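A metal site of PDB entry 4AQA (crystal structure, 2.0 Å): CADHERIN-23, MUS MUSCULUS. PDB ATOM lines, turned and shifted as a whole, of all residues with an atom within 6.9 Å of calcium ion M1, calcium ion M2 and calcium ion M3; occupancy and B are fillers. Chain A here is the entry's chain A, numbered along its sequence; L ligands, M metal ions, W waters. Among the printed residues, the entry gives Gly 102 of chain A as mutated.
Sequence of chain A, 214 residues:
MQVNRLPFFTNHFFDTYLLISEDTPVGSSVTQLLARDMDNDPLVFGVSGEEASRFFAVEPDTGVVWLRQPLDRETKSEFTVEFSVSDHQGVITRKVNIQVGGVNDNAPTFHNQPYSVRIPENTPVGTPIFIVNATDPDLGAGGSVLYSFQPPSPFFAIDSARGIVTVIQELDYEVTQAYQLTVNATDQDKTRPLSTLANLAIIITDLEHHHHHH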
ATOM      1  N   GLU A  22     -16.254 -12.322  13.897  1.00  0.00           N
ATOM      2  CA  GLU A  22     -15.449 -13.081  14.847  1.00  0.00           C
ATOM      3  C   GLU A  22     -13.954 -12.945  14.573  1.00  0.00           C
ATOM      4  O   GLU A  22     -13.142 -13.294  15.435  1.00  0.00           O
ATOM      5  CB  GLU A  22     -15.837 -14.555  14.869  1.00  0.00           C
ATOM      6  CG  GLU A  22     -15.498 -15.353  13.597  1.00  0.00           C
ATOM      7  CD  GLU A  22     -15.691 -16.848  13.763  1.00  0.00           C
ATOM      8  OE1 GLU A  22     -15.496 -17.360  14.884  1.00  0.00           O
ATOM      9  OE2 GLU A  22     -16.011 -17.541  12.760  1.00  0.00           O
ATOM     10  N   LEU A  71     -13.756 -12.868  19.902  1.00  0.00           N
ATOM     11  CA  LEU A  71     -15.051 -13.529  19.762  1.00  0.00           C
ATOM     12  C   LEU A  71     -14.857 -14.831  19.027  1.00  0.00           C
ATOM     13  O   LEU A  71     -13.824 -15.067  18.383  1.00  0.00           O
ATOM     14  CB  LEU A  71     -16.039 -12.647  18.999  1.00  0.00           C
ATOM     15  CG  LEU A  71     -16.257 -11.262  19.597  1.00  0.00           C
ATOM     16  CD1 LEU A  71     -17.147 -10.453  18.669  1.00  0.00           C
ATOM     17  CD2 LEU A  71     -16.853 -11.367  20.995  1.00  0.00           C
ATOM     18  N   ASP A  72     -15.840 -15.709  19.136  1.00  0.00           N
ATOM     19  CA  ASP A  72     -15.806 -16.978  18.460  1.00  0.00           C
ATOM     20  C   ASP A  72     -17.221 -17.412  18.137  1.00  0.00           C
ATOM     21  O   ASP A  72     -17.957 -17.841  19.026  1.00  0.00           O
ATOM     22  CB  ASP A  72     -15.111 -18.024  19.326  1.00  0.00           C
ATOM     23  CG  ASP A  72     -15.023 -19.364  18.657  1.00  0.00           C
ATOM     24  OD1 ASP A  72     -15.500 -19.497  17.483  1.00  0.00           O
ATOM     25  OD2 ASP A  72     -14.483 -20.306  19.285  1.00  0.00           O
ATOM     26  N   ARG A  73     -17.598 -17.325  16.861  1.00  0.00           N
ATOM     27  CA  ARG A  73     -18.943 -17.662  16.439  1.00  0.00           C
ATOM     28  C   ARG A  73     -19.301 -19.119  16.745  1.00  0.00           C
ATOM     29  O   ARG A  73     -20.459 -19.437  17.035  1.00  0.00           O
ATOM     30  CB  ARG A  73     -19.112 -17.390  14.950  1.00  0.00           C
ATOM     31  CG  ARG A  73     -20.552 -17.478  14.509  1.00  0.00           C
ATOM     32  CD  ARG A  73     -20.662 -18.048  13.112  1.00  0.00           C
ATOM     33  NE  ARG A  73     -20.247 -19.434  13.076  1.00  0.00           N
ATOM     34  CZ  ARG A  73     -21.026 -20.473  13.375  1.00  0.00           C
ATOM     35  NH1 ARG A  73     -22.282 -20.287  13.800  1.00  0.00           N
ATOM     36  NH2 ARG A  73     -20.538 -21.694  13.291  1.00  0.00           N
ATOM     37  N   GLU A  74     -18.307 -19.999  16.690  1.00  0.00           N
ATOM     38  CA  GLU A  74     -18.541 -21.412  16.958  1.00  0.00           C
ATOM     39  C   GLU A  74     -18.937 -21.655  18.404  1.00  0.00           C
ATOM     40  O   GLU A  74     -19.642 -22.614  18.683  1.00  0.00           O
ATOM     41  CB  GLU A  74     -17.332 -22.277  16.566  1.00  0.00           C
ATOM     42  CG  GLU A  74     -17.224 -22.578  15.071  1.00  0.00           C
ATOM     43  CD  GLU A  74     -16.970 -21.325  14.223  1.00  0.00           C
ATOM     44  OE1 GLU A  74     -16.050 -20.540  14.561  1.00  0.00           O
ATOM     45  OE2 GLU A  74     -17.706 -21.148  13.200  1.00  0.00           O
ATOM     46  N   THR A  75     -18.491 -20.789  19.312  1.00  0.00           N
ATOM     47  CA  THR A  75     -18.861 -20.889  20.727  1.00  0.00           C
ATOM     48  C   THR A  75     -20.158 -20.140  21.038  1.00  0.00           C
ATOM     49  O   THR A  75     -20.997 -20.645  21.768  1.00  0.00           O
ATOM     50  CB  THR A  75     -17.768 -20.315  21.627  1.00  0.00           C
ATOM     51  OG1 THR A  75     -16.536 -20.992  21.368  1.00  0.00           O
ATOM     52  CG2 THR A  75     -18.149 -20.507  23.101  1.00  0.00           C
ATOM     53  N   GLY A 101     -20.381 -12.373  13.594  1.00  0.00           N
ATOM     54  CA  GLY A 101     -20.225 -12.749  12.196  1.00  0.00           C
ATOM     55  C   GLY A 101     -19.198 -13.850  12.011  1.00  0.00           C
ATOM     56  O   GLY A 101     -18.193 -13.883  12.730  1.00  0.00           O
ATOM     57  N   GLY A 102     -19.442 -14.729  11.043  1.00  0.00           N
ATOM     58  CA  GLY A 102     -18.650 -15.911  10.830  1.00  0.00           C
ATOM     59  C   GLY A 102     -17.573 -15.678   9.811  1.00  0.00           C
ATOM     60  O   GLY A 102     -17.722 -14.874   8.908  1.00  0.00           O
ATOM     61  N   VAL A 103     -16.426 -16.327  10.021  1.00  0.00           N
ATOM     62  CA  VAL A 103     -15.441 -16.477   8.957  1.00  0.00           C
ATOM     63  C   VAL A 103     -14.948 -17.911   9.053  1.00  0.00           C
ATOM     64  O   VAL A 103     -15.108 -18.567  10.063  1.00  0.00           O
ATOM     65  CB  VAL A 103     -14.228 -15.535   9.127  1.00  0.00           C
ATOM     66  CG1 VAL A 103     -14.649 -14.074   9.288  1.00  0.00           C
ATOM     67  CG2 VAL A 103     -13.363 -15.984  10.302  1.00  0.00           C
ATOM     68  N   ASN A 104     -14.336 -18.407   7.990  1.00  0.00           N
ATOM     69  CA  ASN A 104     -13.827 -19.764   7.994  1.00  0.00           C
ATOM     70  C   ASN A 104     -12.558 -19.827   8.844  1.00  0.00           C
ATOM     71  O   ASN A 104     -11.499 -19.335   8.419  1.00  0.00           O
ATOM     72  CB  ASN A 104     -13.537 -20.232   6.579  1.00  0.00           C
ATOM     73  CG  ASN A 104     -13.245 -21.723   6.527  1.00  0.00           C
ATOM     74  OD1 ASN A 104     -13.986 -22.525   7.098  1.00  0.00           O
ATOM     75  ND2 ASN A 104     -12.151 -22.096   5.868  1.00  0.00           N
ATOM     76  N   ASP A 105     -12.671 -20.389  10.046  1.00  0.00           N
ATOM     77  CA  ASP A 105     -11.483 -20.547  10.891  1.00  0.00           C
ATOM     78  C   ASP A 105     -11.270 -21.918  11.515  1.00  0.00           C
ATOM     79  O   ASP A 105     -10.423 -22.076  12.389  1.00  0.00           O
ATOM     80  CB  ASP A 105     -11.380 -19.406  11.925  1.00  0.00           C
ATOM     81  CG  ASP A 105     -12.571 -19.308  12.883  1.00  0.00           C
ATOM     82  OD1 ASP A 105     -13.623 -19.973  12.695  1.00  0.00           O
ATOM     83  OD2 ASP A 105     -12.459 -18.517  13.859  1.00  0.00           O
ATOM     84  N   ASN A 106     -11.979 -22.940  11.041  1.00  0.00           N
ATOM     85  CA  ASN A 106     -11.685 -24.323  11.430  1.00  0.00           C
ATOM     86  C   ASN A 106     -11.443 -25.208  10.217  1.00  0.00           C
ATOM     87  O   ASN A 106     -12.014 -24.968   9.155  1.00  0.00           O
ATOM     88  CB  ASN A 106     -12.831 -24.935  12.237  1.00  0.00           C
ATOM     89  CG  ASN A 106     -13.143 -24.151  13.499  1.00  0.00           C
ATOM     90  OD1 ASN A 106     -12.727 -24.562  14.589  1.00  0.00           O
ATOM     91  ND2 ASN A 106     -13.850 -23.018  13.378  1.00  0.00           N
ATOM     92  N   ALA A 107     -10.590 -26.216  10.392  1.00  0.00           N
ATOM     93  CA  ALA A 107     -10.413 -27.225   9.369  1.00  0.00           C
ATOM     94  C   ALA A 107     -11.342 -28.348   9.764  1.00  0.00           C
ATOM     95  O   ALA A 107     -11.781 -28.362  10.900  1.00  0.00           O
ATOM     96  CB  ALA A 107      -8.967 -27.709   9.333  1.00  0.00           C
ATOM     97  N   PRO A 108     -11.668 -29.252   8.837  1.00  0.00           N
ATOM     98  CA  PRO A 108     -12.455 -30.436   9.205  1.00  0.00           C
ATOM     99  C   PRO A 108     -11.759 -31.376  10.185  1.00  0.00           C
ATOM    100  O   PRO A 108     -10.533 -31.371  10.293  1.00  0.00           O
ATOM    101  CB  PRO A 108     -12.701 -31.142   7.869  1.00  0.00           C
ATOM    102  CG  PRO A 108     -12.460 -30.106   6.824  1.00  0.00           C
ATOM    103  CD  PRO A 108     -11.395 -29.218   7.386  1.00  0.00           C
ATOM    104  N   ASP A 136     -17.095 -30.175  10.059  1.00  0.00           N
ATOM    105  CA  ASP A 136     -16.461 -28.846  10.138  1.00  0.00           C
ATOM    106  C   ASP A 136     -17.526 -27.890  10.638  1.00  0.00           C
ATOM    107  O   ASP A 136     -18.562 -27.811  10.017  1.00  0.00           O
ATOM    108  CB  ASP A 136     -15.998 -28.439   8.749  1.00  0.00           C
ATOM    109  CG  ASP A 136     -15.197 -27.140   8.752  1.00  0.00           C
ATOM    110  OD1 ASP A 136     -15.567 -26.165   9.478  1.00  0.00           O
ATOM    111  OD2 ASP A 136     -14.183 -27.098   8.005  1.00  0.00           O
ATOM    112  N   PRO A 137     -17.268 -27.165  11.744  1.00  0.00           N
ATOM    113  CA  PRO A 137     -18.289 -26.350  12.415  1.00  0.00           C
ATOM    114  C   PRO A 137     -18.534 -24.922  11.841  1.00  0.00           C
ATOM    115  O   PRO A 137     -19.447 -24.246  12.287  1.00  0.00           O
ATOM    116  CB  PRO A 137     -17.745 -26.258  13.832  1.00  0.00           C
ATOM    117  CG  PRO A 137     -16.266 -26.198  13.612  1.00  0.00           C
ATOM    118  CD  PRO A 137     -16.000 -27.154  12.489  1.00  0.00           C
ATOM    119  N   ASP A 138     -17.746 -24.499  10.864  1.00  0.00           N
ATOM    120  CA  ASP A 138     -17.927 -23.168  10.282  1.00  0.00           C
ATOM    121  C   ASP A 138     -19.208 -23.116   9.450  1.00  0.00           C
ATOM    122  O   ASP A 138     -19.715 -24.145   9.020  1.00  0.00           O
ATOM    123  CB  ASP A 138     -16.740 -22.762   9.406  1.00  0.00           C
ATOM    124  CG  ASP A 138     -15.417 -22.694  10.175  1.00  0.00           C
ATOM    125  OD1 ASP A 138     -15.305 -21.889  11.155  1.00  0.00           O
ATOM    126  OD2 ASP A 138     -14.496 -23.430   9.771  1.00  0.00           O
ATOM    127  N   LEU A 139     -19.709 -21.904   9.240  1.00  0.00           N
ATOM    128  CA  LEU A 139     -20.934 -21.698   8.484  1.00  0.00           C
ATOM    129  C   LEU A 139     -20.712 -21.933   6.988  1.00  0.00           C
ATOM    130  O   LEU A 139     -19.636 -21.634   6.439  1.00  0.00           O
ATOM    131  CB  LEU A 139     -21.481 -20.290   8.695  1.00  0.00           C
ATOM    132  CG  LEU A 139     -22.119 -19.946  10.038  1.00  0.00           C
ATOM    133  CD1 LEU A 139     -22.689 -18.548   9.962  1.00  0.00           C
ATOM    134  CD2 LEU A 139     -23.218 -20.932  10.415  1.00  0.00           C
ATOM    135  N   ALA A 141     -20.181 -22.586   3.160  1.00  0.00           N
ATOM    136  CA  ALA A 141     -19.173 -23.238   2.340  1.00  0.00           C
ATOM    137  C   ALA A 141     -18.001 -23.674   3.200  1.00  0.00           C
ATOM    138  O   ALA A 141     -17.393 -24.720   2.976  1.00  0.00           O
ATOM    139  CB  ALA A 141     -18.709 -22.327   1.204  1.00  0.00           C
ATOM    140  N   GLY A 142     -17.686 -22.857   4.201  1.00  0.00           N
ATOM    141  CA  GLY A 142     -16.612 -23.181   5.110  1.00  0.00           C
ATOM    142  C   GLY A 142     -16.902 -24.380   5.985  1.00  0.00           C
ATOM    143  O   GLY A 142     -16.015 -24.826   6.669  1.00  0.00           O
ATOM    144  N   GLY A 143     -18.130 -24.891   5.974  1.00  0.00           N
ATOM    145  CA  GLY A 143     -18.493 -26.041   6.776  1.00  0.00           C
ATOM    146  C   GLY A 143     -18.868 -27.267   5.975  1.00  0.00           C
ATOM    147  O   GLY A 143     -19.246 -28.289   6.558  1.00  0.00           O
ATOM    148  N   SER A 144     -18.777 -27.189   4.640  1.00  0.00           N
ATOM    149  CA  SER A 144     -19.211 -28.256   3.760  1.00  0.00           C
ATOM    150  C   SER A 144     -17.970 -28.974   3.246  1.00  0.00           C
ATOM    151  O   SER A 144     -17.083 -28.356   2.650  1.00  0.00           O
ATOM    152  CB  SER A 144     -20.056 -27.678   2.616  1.00  0.00           C
ATOM    153  OG  SER A 144     -20.418 -28.684   1.662  1.00  0.00           O
ATOM    154  N   THR A 186     -11.412 -31.301   2.916  1.00  0.00           N
ATOM    155  CA  THR A 186     -11.324 -29.839   2.829  1.00  0.00           C
ATOM    156  C   THR A 186     -12.705 -29.222   2.902  1.00  0.00           C
ATOM    157  O   THR A 186     -13.705 -29.803   2.411  1.00  0.00           O
ATOM    158  CB  THR A 186     -10.612 -29.323   1.541  1.00  0.00           C
ATOM    159  OG1 THR A 186     -10.555 -27.881   1.557  1.00  0.00           O
ATOM    160  CG2 THR A 186     -11.347 -29.717   0.270  1.00  0.00           C
ATOM    161  N   ASP A 187     -12.774 -28.062   3.525  1.00  0.00           N
ATOM    162  CA  ASP A 187     -13.968 -27.233   3.370  1.00  0.00           C
ATOM    163  C   ASP A 187     -13.885 -26.502   2.033  1.00  0.00           C
ATOM    164  O   ASP A 187     -12.924 -26.678   1.268  1.00  0.00           O
ATOM    165  CB  ASP A 187     -14.226 -26.324   4.576  1.00  0.00           C
ATOM    166  CG  ASP A 187     -13.106 -25.296   4.809  1.00  0.00           C
ATOM    167  OD1 ASP A 187     -12.583 -24.761   3.823  1.00  0.00           O
ATOM    168  OD2 ASP A 187     -12.790 -25.049   6.001  1.00  0.00           O
ATOM    169  N   GLN A 188     -14.940 -25.763   1.718  1.00  0.00           N
ATOM    170  CA  GLN A 188     -15.074 -25.098   0.444  1.00  0.00           C
ATOM    171  C   GLN A 188     -15.105 -23.573   0.569  1.00  0.00           C
ATOM    172  O   GLN A 188     -15.650 -22.916  -0.279  1.00  0.00           O
ATOM    173  CB  GLN A 188     -16.359 -25.581  -0.222  1.00  0.00           C
ATOM    174  CG  GLN A 188     -16.277 -27.023  -0.650  1.00  0.00           C
ATOM    175  CD  GLN A 188     -17.539 -27.514  -1.284  1.00  0.00           C
ATOM    176  OE1 GLN A 188     -17.713 -27.416  -2.501  1.00  0.00           O
ATOM    177  NE2 GLN A 188     -18.444 -28.055  -0.467  1.00  0.00           N
ATOM    178  N   ASP A 189     -14.516 -23.012   1.610  1.00  0.00           N
ATOM    179  CA  ASP A 189     -14.470 -21.564   1.699  1.00  0.00           C
ATOM    180  C   ASP A 189     -13.779 -21.022   0.433  1.00  0.00           C
ATOM    181  O   ASP A 189     -12.826 -21.625  -0.060  1.00  0.00           O
ATOM    182  CB  ASP A 189     -13.697 -21.130   2.941  1.00  0.00           C
ATOM    183  CG  ASP A 189     -13.805 -19.652   3.172  1.00  0.00           C
ATOM    184  OD1 ASP A 189     -14.932 -19.150   3.411  1.00  0.00           O
ATOM    185  OD2 ASP A 189     -12.764 -18.974   3.133  1.00  0.00           O
ATOM    186  N   ARG A 192     -10.212 -18.744   1.856  1.00  0.00           N
ATOM    187  CA  ARG A 192      -9.286 -19.415   2.768  1.00  0.00           C
ATOM    188  C   ARG A 192      -9.758 -20.839   3.088  1.00  0.00           C
ATOM    189  O   ARG A 192     -10.162 -21.115   4.218  1.00  0.00           O
ATOM    190  CB  ARG A 192      -9.127 -18.609   4.065  1.00  0.00           C
ATOM    191  CG  ARG A 192      -8.564 -17.212   3.849  1.00  0.00           C
ATOM    192  CD  ARG A 192      -8.404 -16.387   5.125  1.00  0.00           C
ATOM    193  NE  ARG A 192      -7.525 -17.076   6.066  1.00  0.00           N
ATOM    194  CZ  ARG A 192      -7.923 -17.837   7.092  1.00  0.00           C
ATOM    195  NH1 ARG A 192      -9.200 -18.018   7.376  1.00  0.00           N
ATOM    196  NH2 ARG A 192      -6.998 -18.443   7.834  1.00  0.00           N
ATOM    197  N   PRO A 193      -9.720 -21.745   2.102  1.00  0.00           N
ATOM    198  CA  PRO A 193     -10.137 -23.112   2.410  1.00  0.00           C
ATOM    199  C   PRO A 193      -9.147 -23.782   3.365  1.00  0.00           C
ATOM    200  O   PRO A 193      -7.927 -23.494   3.337  1.00  0.00           O
ATOM    201  CB  PRO A 193     -10.144 -23.807   1.059  1.00  0.00           C
ATOM    202  CG  PRO A 193      -9.139 -23.045   0.266  1.00  0.00           C
ATOM    203  CD  PRO A 193      -9.285 -21.616   0.699  1.00  0.00           C
ATOM    204  N   LEU A 194      -9.684 -24.644   4.226  1.00  0.00           N
ATOM    205  CA  LEU A 194      -8.890 -25.311   5.220  1.00  0.00           C
ATOM    206  C   LEU A 194      -9.118 -26.807   5.098  1.00  0.00           C
ATOM    207  O   LEU A 194     -10.226 -27.237   4.747  1.00  0.00           O
ATOM    208  CB  LEU A 194      -9.240 -24.799   6.616  1.00  0.00           C
ATOM    209  CG  LEU A 194      -8.853 -23.346   6.927  1.00  0.00           C
ATOM    210  CD1 LEU A 194      -9.377 -22.927   8.296  1.00  0.00           C
ATOM    211  CD2 LEU A 194      -7.350 -23.161   6.859  1.00  0.00           C
HETATM  212 CL1  LIG L   1     -18.183 -19.323  10.361  1.00  0.00          CL
HETATM  213 CA    CA M   1     -14.181 -19.281  15.299  1.00  0.00          CA
HETATM  214 CA    CA M   2     -15.910 -19.730  11.963  1.00  0.00          CA
HETATM  215 CA    CA M   3     -14.027 -24.778   7.952  1.00  0.00          CA
HETATM  216  O   HOH W   1     -12.629 -18.184  16.809  1.00  0.00           O
HETATM  217  O   HOH W   2     -13.064 -21.202  15.704  1.00  0.00           O
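Calcium ion M3 is bound by the side-chain carboxylate (OD2) of Asp 138 (2.3 Å), the side-chain carboxylate (OD2) of Asp 136 (2.3 Å), the side-chain carboxylate (OD2) of Asp 187 (2.3 Å), the backbone carbonyl oxygen (O) of Asn 106 (2.4 Å), the backbone carbonyl oxygen (O) of Gly 142 (2.4 Å), the side-chain amide oxygen (OD1) of Asn 104 (2.4 Å) and the side-chain carboxylate (OD1) of Asp 136 (2.6 Å). Calcium ion M3 has seven donor atoms within binding distance.
OD1 of Asp 187 sits at hydrogen-bond distance from N of Leu 194, 2.9 Å away. OD1 of Asp 187 lies within hydrogen-bond range of N of Asp 189 (3.4 Å). The side-chain carboxylate (OE1) of Glu 22 lies close to the backbone NH (N) of Arg 73 (2.9 Å). O of Gly 101 lies within hydrogen-bond range of N of Glu 22. ND2 of Asn 106 lies close to OD1 of Asp 105 (3.1 Å). OE2 of Glu 74 lies close to NH2 of Arg 73, at 2.9 Å. ND2 of Asn 104 sits at hydrogen-bond distance from O of Arg 192, at 2.8 Å. OG1 of Thr 75 is in hydrogen-bond range of OD2 of Asp 72 (3.0 Å).
Four residues have an atom within 4 Å of calcium ion M1: Glu 22, Asp 72, Glu 74 and Asp 105. The nearest printed residue that does not touch calcium ion M1 is Asn 106 (4.2 Å).
Calcium ion M1 is bound by water W2, the side-chain carboxylate (OE1) of Glu 22, the side-chain carboxylate (OE1) of Glu 74, the side-chain carboxylate (OD2) of Asp 105, water W1, the side-chain carboxylate (OD1) of Asp 72 and the side-chain carboxylate (OD1) of Asp 105.
Within 4 Å of calcium ion M3: Asn 104, Asn 106, Asp 136, Asp 138, Gly 142 and Asp 187.
Within 4 Å of calcium ion M2: Glu 22, Glu 74, Val 103, Asp 105 and Asp 138.
Calcium ion M2 is bound by OE2 of Glu 22 (2.3 Å), O of Val 103 (2.4 Å), OD1 of Asp 138 (2.4 Å), OD1 of Asp 105 (2.4 Å), OE2 of Glu 74 (2.6 Å), OE1 of Glu 74 (2.7 Å) and CL1 of the ligand (2.8 Å).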
